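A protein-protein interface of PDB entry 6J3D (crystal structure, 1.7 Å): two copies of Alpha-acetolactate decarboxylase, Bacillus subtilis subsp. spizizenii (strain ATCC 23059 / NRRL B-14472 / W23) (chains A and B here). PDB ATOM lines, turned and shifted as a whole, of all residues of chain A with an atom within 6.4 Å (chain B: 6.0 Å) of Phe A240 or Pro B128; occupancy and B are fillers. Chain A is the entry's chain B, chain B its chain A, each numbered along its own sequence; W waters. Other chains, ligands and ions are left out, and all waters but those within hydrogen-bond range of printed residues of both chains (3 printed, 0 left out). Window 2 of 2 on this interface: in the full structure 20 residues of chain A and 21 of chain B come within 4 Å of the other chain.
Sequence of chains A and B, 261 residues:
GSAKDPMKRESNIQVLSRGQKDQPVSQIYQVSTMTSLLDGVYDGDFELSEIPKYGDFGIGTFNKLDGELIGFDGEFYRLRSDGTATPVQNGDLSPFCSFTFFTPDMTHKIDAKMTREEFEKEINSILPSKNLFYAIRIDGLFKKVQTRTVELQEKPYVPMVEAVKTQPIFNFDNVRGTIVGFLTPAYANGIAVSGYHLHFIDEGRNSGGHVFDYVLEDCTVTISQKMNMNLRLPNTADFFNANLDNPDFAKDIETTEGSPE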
ATOM      1  N   PRO A 234      11.324  18.100  -8.229  1.00  0.00           N
ATOM      2  CA  PRO A 234      10.561  17.420  -7.189  1.00  0.00           C
ATOM      3  C   PRO A 234       9.316  18.136  -6.754  1.00  0.00           C
ATOM      4  O   PRO A 234       9.307  19.360  -6.710  1.00  0.00           O
ATOM      5  CB  PRO A 234      11.525  17.327  -6.024  1.00  0.00           C
ATOM      6  CG  PRO A 234      12.521  18.320  -6.254  1.00  0.00           C
ATOM      7  CD  PRO A 234      12.576  18.677  -7.726  1.00  0.00           C
ATOM      8  N   ASN A 235       8.295  17.374  -6.391  1.00  0.00           N
ATOM      9  CA  ASN A 235       7.042  17.953  -5.918  1.00  0.00           C
ATOM     10  C   ASN A 235       7.015  17.954  -4.405  1.00  0.00           C
ATOM     11  O   ASN A 235       6.089  17.428  -3.794  1.00  0.00           O
ATOM     12  CB  ASN A 235       5.870  17.156  -6.503  1.00  0.00           C
ATOM     13  CG  ASN A 235       4.559  17.880  -6.385  1.00  0.00           C
ATOM     14  OD1 ASN A 235       4.504  19.112  -6.284  1.00  0.00           O
ATOM     15  ND2 ASN A 235       3.474  17.116  -6.393  1.00  0.00           N
ATOM     16  N   THR A 236       8.012  18.608  -3.808  1.00  0.00           N
ATOM     17  CA  THR A 236       8.156  18.623  -2.356  1.00  0.00           C
ATOM     18  C   THR A 236       8.185  20.059  -1.828  1.00  0.00           C
ATOM     19  O   THR A 236       8.657  20.986  -2.472  1.00  0.00           O
ATOM     20  CB  THR A 236       9.389  17.927  -1.928  1.00  0.00           C
ATOM     21  OG1 THR A 236      10.525  18.641  -2.426  1.00  0.00           O
ATOM     22  CG2 THR A 236       9.398  16.489  -2.461  1.00  0.00           C
ATOM     23  N   ALA A 237       7.690  20.232  -0.619  1.00  0.00           N
ATOM     24  CA  ALA A 237       7.759  21.518   0.046  1.00  0.00           C
ATOM     25  C   ALA A 237       9.222  21.915   0.227  1.00  0.00           C
ATOM     26  O   ALA A 237       9.563  23.056   0.060  1.00  0.00           O
ATOM     27  CB  ALA A 237       7.049  21.415   1.397  1.00  0.00           C
ATOM     28  N   ASP A 238      10.083  20.955   0.574  1.00  0.00           N
ATOM     29  CA  ASP A 238      11.516  21.196   0.776  1.00  0.00           C
ATOM     30  C   ASP A 238      12.163  21.829  -0.467  1.00  0.00           C
ATOM     31  O   ASP A 238      12.886  22.824  -0.351  1.00  0.00           O
ATOM     32  CB  ASP A 238      12.261  19.915   1.130  1.00  0.00           C
ATOM     33  CG  ASP A 238      12.018  19.430   2.549  1.00  0.00           C
ATOM     34  OD1 ASP A 238      11.505  20.173   3.437  1.00  0.00           O
ATOM     35  OD2 ASP A 238      12.396  18.273   2.740  1.00  0.00           O
ATOM     36  N   PHE A 239      11.822  21.337  -1.654  1.00  0.00           N
ATOM     37  CA  PHE A 239      12.339  21.947  -2.885  1.00  0.00           C
ATOM     38  C   PHE A 239      11.620  23.258  -3.194  1.00  0.00           C
ATOM     39  O   PHE A 239      12.274  24.234  -3.586  1.00  0.00           O
ATOM     40  CB  PHE A 239      12.247  20.975  -4.065  1.00  0.00           C
ATOM     41  CG  PHE A 239      12.820  21.532  -5.346  1.00  0.00           C
ATOM     42  CD1 PHE A 239      14.157  21.501  -5.618  1.00  0.00           C
ATOM     43  CD2 PHE A 239      11.968  22.138  -6.278  1.00  0.00           C
ATOM     44  CE1 PHE A 239      14.674  22.067  -6.789  1.00  0.00           C
ATOM     45  CE2 PHE A 239      12.485  22.694  -7.429  1.00  0.00           C
ATOM     46  CZ  PHE A 239      13.805  22.667  -7.696  1.00  0.00           C
ATOM     47  N   PHE A 240      10.290  23.283  -3.062  1.00  0.00           N
ATOM     48  CA  PHE A 240       9.552  24.476  -3.413  1.00  0.00           C
ATOM     49  C   PHE A 240      10.044  25.659  -2.579  1.00  0.00           C
ATOM     50  O   PHE A 240      10.110  26.765  -3.083  1.00  0.00           O
ATOM     51  CB  PHE A 240       8.047  24.348  -3.181  1.00  0.00           C
ATOM     52  CG  PHE A 240       7.282  23.679  -4.298  1.00  0.00           C
ATOM     53  CD1 PHE A 240       7.798  22.610  -4.980  1.00  0.00           C
ATOM     54  CD2 PHE A 240       5.986  24.081  -4.567  1.00  0.00           C
ATOM     55  CE1 PHE A 240       7.061  21.976  -5.950  1.00  0.00           C
ATOM     56  CE2 PHE A 240       5.244  23.455  -5.569  1.00  0.00           C
ATOM     57  CZ  PHE A 240       5.788  22.381  -6.224  1.00  0.00           C
ATOM     58  N   ASN A 241      10.349  25.432  -1.289  1.00  0.00           N
ATOM     59  CA  ASN A 241      10.645  26.526  -0.373  1.00  0.00           C
ATOM     60  C   ASN A 241      12.143  26.820  -0.275  1.00  0.00           C
ATOM     61  O   ASN A 241      12.521  27.786   0.390  1.00  0.00           O
ATOM     62  CB  ASN A 241      10.110  26.211   1.039  1.00  0.00           C
ATOM     63  CG  ASN A 241       8.602  26.076   1.090  1.00  0.00           C
ATOM     64  OD1 ASN A 241       7.894  26.792   0.391  1.00  0.00           O
ATOM     65  ND2 ASN A 241       8.104  25.178   1.933  1.00  0.00           N
ATOM     66  N   ALA A 242      12.973  26.020  -0.910  1.00  0.00           N
ATOM     67  CA  ALA A 242      14.433  26.180  -0.835  1.00  0.00           C
ATOM     68  C   ALA A 242      14.903  27.496  -1.425  1.00  0.00           C
ATOM     69  O   ALA A 242      14.425  27.915  -2.491  1.00  0.00           O
ATOM     70  CB  ALA A 242      15.124  25.001  -1.535  1.00  0.00           C
ATOM     71  N   ASN A 243      15.801  28.171  -0.713  1.00  0.00           N
ATOM     72  CA  ASN A 243      16.549  29.306  -1.235  1.00  0.00           C
ATOM     73  C   ASN A 243      17.721  28.828  -2.084  1.00  0.00           C
ATOM     74  O   ASN A 243      18.762  28.362  -1.582  1.00  0.00           O
ATOM     75  CB  ASN A 243      17.036  30.247  -0.100  1.00  0.00           C
ATOM     76  CG  ASN A 243      17.670  31.529  -0.638  1.00  0.00           C
ATOM     77  OD1 ASN A 243      17.773  31.738  -1.861  1.00  0.00           O
ATOM     78  ND2 ASN A 243      18.032  32.426   0.264  1.00  0.00           N
ATOM     79  N   MET B 106      -3.446  28.910 -12.466  1.00  0.00           N
ATOM     80  CA  MET B 106      -3.780  30.091 -11.673  1.00  0.00           C
ATOM     81  C   MET B 106      -4.324  31.155 -12.611  1.00  0.00           C
ATOM     82  O   MET B 106      -3.815  31.304 -13.733  1.00  0.00           O
ATOM     83  CB  MET B 106      -2.538  30.650 -10.966  1.00  0.00           C
ATOM     84  CG  MET B 106      -1.922  29.740  -9.895  1.00  0.00           C
ATOM     85  SD  MET B 106      -0.155  30.059  -9.541  1.00  0.00           S
ATOM     86  CE  MET B 106       0.675  29.065 -10.774  1.00  0.00           C
ATOM     87  N   ILE B 126       2.593  35.403  -5.748  1.00  0.00           N
ATOM     88  CA  ILE B 126       1.571  34.379  -5.786  1.00  0.00           C
ATOM     89  C   ILE B 126       2.068  33.033  -6.312  1.00  0.00           C
ATOM     90  O   ILE B 126       1.357  32.049  -6.238  1.00  0.00           O
ATOM     91  CB  ILE B 126       0.329  34.832  -6.546  1.00  0.00           C
ATOM     92  CG1 ILE B 126       0.622  35.057  -8.025  1.00  0.00           C
ATOM     93  CG2 ILE B 126      -0.275  36.069  -5.815  1.00  0.00           C
ATOM     94  CD1 ILE B 126      -0.635  35.401  -8.882  1.00  0.00           C
ATOM     95  N   LEU B 127       3.282  32.985  -6.833  1.00  0.00           N
ATOM     96  CA  LEU B 127       3.830  31.707  -7.304  1.00  0.00           C
ATOM     97  C   LEU B 127       4.075  30.752  -6.127  1.00  0.00           C
ATOM     98  O   LEU B 127       4.521  31.172  -5.055  1.00  0.00           O
ATOM     99  CB  LEU B 127       5.156  31.933  -8.060  1.00  0.00           C
ATOM    100  CG  LEU B 127       5.140  32.723  -9.378  1.00  0.00           C
ATOM    101  CD1 LEU B 127       6.588  32.863  -9.871  1.00  0.00           C
ATOM    102  CD2 LEU B 127       4.240  32.087 -10.452  1.00  0.00           C
ATOM    103  N   PRO B 128       3.820  29.441  -6.335  1.00  0.00           N
ATOM    104  CA  PRO B 128       4.090  28.468  -5.286  1.00  0.00           C
ATOM    105  C   PRO B 128       5.564  28.340  -4.956  1.00  0.00           C
ATOM    106  O   PRO B 128       5.882  27.964  -3.846  1.00  0.00           O
ATOM    107  CB  PRO B 128       3.574  27.150  -5.846  1.00  0.00           C
ATOM    108  CG  PRO B 128       2.906  27.430  -7.101  1.00  0.00           C
ATOM    109  CD  PRO B 128       3.009  28.877  -7.428  1.00  0.00           C
ATOM    110  N   SER B 129       6.432  28.653  -5.919  1.00  0.00           N
ATOM    111  CA  SER B 129       7.869  28.574  -5.720  1.00  0.00           C
ATOM    112  C   SER B 129       8.590  29.322  -6.831  1.00  0.00           C
ATOM    113  O   SER B 129       8.203  29.231  -7.977  1.00  0.00           O
ATOM    114  CB  SER B 129       8.299  27.123  -5.804  1.00  0.00           C
ATOM    115  OG  SER B 129       9.718  26.997  -5.698  1.00  0.00           O
ATOM    116  N   LYS B 130       9.666  29.997  -6.461  1.00  0.00           N
ATOM    117  CA  LYS B 130      10.615  30.592  -7.405  1.00  0.00           C
ATOM    118  C   LYS B 130      11.504  29.549  -8.083  1.00  0.00           C
ATOM    119  O   LYS B 130      12.253  29.904  -8.970  1.00  0.00           O
ATOM    120  CB  LYS B 130      11.610  31.459  -6.590  1.00  0.00           C
ATOM    121  N   ASN B 131      11.436  28.288  -7.671  1.00  0.00           N
ATOM    122  CA  ASN B 131      12.330  27.270  -8.209  1.00  0.00           C
ATOM    123  C   ASN B 131      11.731  26.411  -9.315  1.00  0.00           C
ATOM    124  O   ASN B 131      12.351  25.445  -9.745  1.00  0.00           O
ATOM    125  CB  ASN B 131      12.826  26.362  -7.085  1.00  0.00           C
ATOM    126  CG  ASN B 131      13.441  27.165  -5.939  1.00  0.00           C
ATOM    127  OD1 ASN B 131      14.115  28.156  -6.197  1.00  0.00           O
ATOM    128  ND2 ASN B 131      13.236  26.735  -4.677  1.00  0.00           N
ATOM    129  N   LEU B 132      10.529  26.752  -9.759  1.00  0.00           N
ATOM    130  CA  LEU B 132       9.864  25.978 -10.792  1.00  0.00           C
ATOM    131  C   LEU B 132       9.836  26.798 -12.082  1.00  0.00           C
ATOM    132  O   LEU B 132      10.115  27.990 -12.080  1.00  0.00           O
ATOM    133  CB  LEU B 132       8.437  25.632 -10.392  1.00  0.00           C
ATOM    134  CG  LEU B 132       8.223  24.944  -9.045  1.00  0.00           C
ATOM    135  CD1 LEU B 132       6.718  24.775  -8.757  1.00  0.00           C
ATOM    136  CD2 LEU B 132       8.933  23.604  -9.053  1.00  0.00           C
ATOM    137  N   TYR B 134       7.389  28.295 -15.184  1.00  0.00           N
ATOM    138  CA  TYR B 134       5.971  28.668 -15.459  1.00  0.00           C
ATOM    139  C   TYR B 134       5.827  29.192 -16.847  1.00  0.00           C
ATOM    140  O   TYR B 134       6.735  29.782 -17.393  1.00  0.00           O
ATOM    141  CB  TYR B 134       5.464  29.750 -14.510  1.00  0.00           C
ATOM    142  CG  TYR B 134       5.609  29.391 -13.035  1.00  0.00           C
ATOM    143  CD1 TYR B 134       6.782  29.661 -12.344  1.00  0.00           C
ATOM    144  CD2 TYR B 134       4.579  28.772 -12.353  1.00  0.00           C
ATOM    145  CE1 TYR B 134       6.934  29.293 -11.006  1.00  0.00           C
ATOM    146  CE2 TYR B 134       4.737  28.402 -11.021  1.00  0.00           C
ATOM    147  CZ  TYR B 134       5.893  28.667 -10.374  1.00  0.00           C
ATOM    148  OH  TYR B 134       6.082  28.327  -9.056  1.00  0.00           O
ATOM    149  N   GLN B 225       2.020  25.986 -14.296  1.00  0.00           N
ATOM    150  CA  GLN B 225       3.211  25.542 -13.583  1.00  0.00           C
ATOM    151  C   GLN B 225       3.785  24.335 -14.280  1.00  0.00           C
ATOM    152  O   GLN B 225       3.048  23.407 -14.564  1.00  0.00           O
ATOM    153  CB  GLN B 225       2.785  25.183 -12.132  1.00  0.00           C
ATOM    154  CG  GLN B 225       3.790  24.536 -11.268  1.00  0.00           C
ATOM    155  CD  GLN B 225       3.220  24.160  -9.886  1.00  0.00           C
ATOM    156  OE1 GLN B 225       2.377  24.863  -9.376  1.00  0.00           O
ATOM    157  NE2 GLN B 225       3.664  23.028  -9.317  1.00  0.00           N
ATOM    158  N   MET B 227       6.861  21.227 -14.280  1.00  0.00           N
ATOM    159  CA  MET B 227       7.769  20.522 -13.346  1.00  0.00           C
ATOM    160  C   MET B 227       8.944  19.881 -14.099  1.00  0.00           C
ATOM    161  O   MET B 227       9.804  19.248 -13.487  1.00  0.00           O
ATOM    162  CB  MET B 227       7.016  19.416 -12.607  1.00  0.00           C
ATOM    163  CG  MET B 227       5.883  19.901 -11.749  1.00  0.00           C
ATOM    164  SD  MET B 227       6.456  21.105 -10.526  1.00  0.00           S
ATOM    165  CE  MET B 227       7.125  20.055  -9.261  1.00  0.00           C
HETATM  166  O   HOH W   1       2.644  21.039  -7.289  1.00  0.00           O
HETATM  167  O   HOH W   2      10.574  29.552  -3.610  1.00  0.00           O
HETATM  168  O   HOH W   3      15.317  30.057  -4.711  1.00  0.00           O
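ND2 of Asn B131 sits at hydrogen-bond distance from O of Ala A242, 2.8 Å away.
OG of Ser B129 lies within hydrogen-bond range of O of Phe A240, 2.7 Å away.
The side-chain amide nitrogen (ND2) of Asn B131 sits at hydrogen-bond distance from the backbone carbonyl oxygen (O) of Phe A239 (2.9 Å).
N of Asn B131 lies within hydrogen-bond range of OG of Ser B129, 2.9 Å away.
NE2 of Gln B225 is in hydrogen-bond range of SD of Met B227.
The side-chain hydroxyl (OG1) of Thr A236 lies within hydrogen-bond range of the backbone NH (N) of Phe A239.
The side-chain hydroxyl (OH) of Tyr B134 sits at hydrogen-bond distance from the backbone carbonyl oxygen (O) of Ser B129 (2.5 Å).
O of Pro A234 touches CE of Met B227, at 3.4 Å.
CA of Asn A235 touches CE of Met B227, 3.9 Å away.
CD2 of Phe A240 touches O of Pro B128, 3.95 Å away.
Asn B131 touches Phe A240.
Phe A240 touches Leu B132 (CZ to CD1, 3.6 Å).
Gln B225 touches Phe A240.
CE1 of Phe A240 touches CE of Met B227, 3.8 Å away.
Of the printed residues of chain B, Pro A234 touches Met B227 (3.4 Å).
Of the printed residues of chain B, Phe A239 touches Asn B131.
Of chain B, only Pro B128, Ser B129, Asn B131, Leu B132, Gln B225 and Met B227 come within 4 Å of Phe A240.
Printed residues of chain B within 4 Å of Ala A242: Asn B131.
Pro B128 touches just one residue of chain A: Phe A240.
Of the printed residues of chain A, Asn B131 touches Phe A239 (2.9 Å), Phe A240 (3.5 Å) and Ala A242 (2.8 Å).
Tyr B134 touches none of the printed residues of chain A.
The nearest residue of chain B that does not touch Phe A240 is Lys B130 (4.7 Å).
The nearest printed residue of chain B that does not touch Ala A242 is Ser B129 (5.8 Å).
Along chain B the printed residues that touch a printed residue of chain A span positions 128 to 227.
Hydrophobic or aromatic side chains of chain A within 4 Å of the printed part of chain B: Phe A239 and Phe A240.
Among the printed residues, no Asp or Glu carboxylate lies within 4 Å of a Lys or Arg side-chain nitrogen of the other chain.
No position is printed for both chains.
Of the 10 pairs that touch across the chains among the printed residues, none has its exchanged pair printed and touching as well.
Water W3 lies within hydrogen-bond range of OD1 of Asn B131 (2.7 Å) and O of Ala A242 (3.2 Å).
Water W1 lies within hydrogen-bond range of the side-chain amide oxygen of Asn A235 (2.9 Å) and the side-chain amide nitrogen of Gln B225 (3.0 Å).
Water W2 lies within hydrogen-bond range of O of Phe A240 (2.9 Å), N of Lys B130 (3.0 Å) and OG of Ser B129 (3.4 Å).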
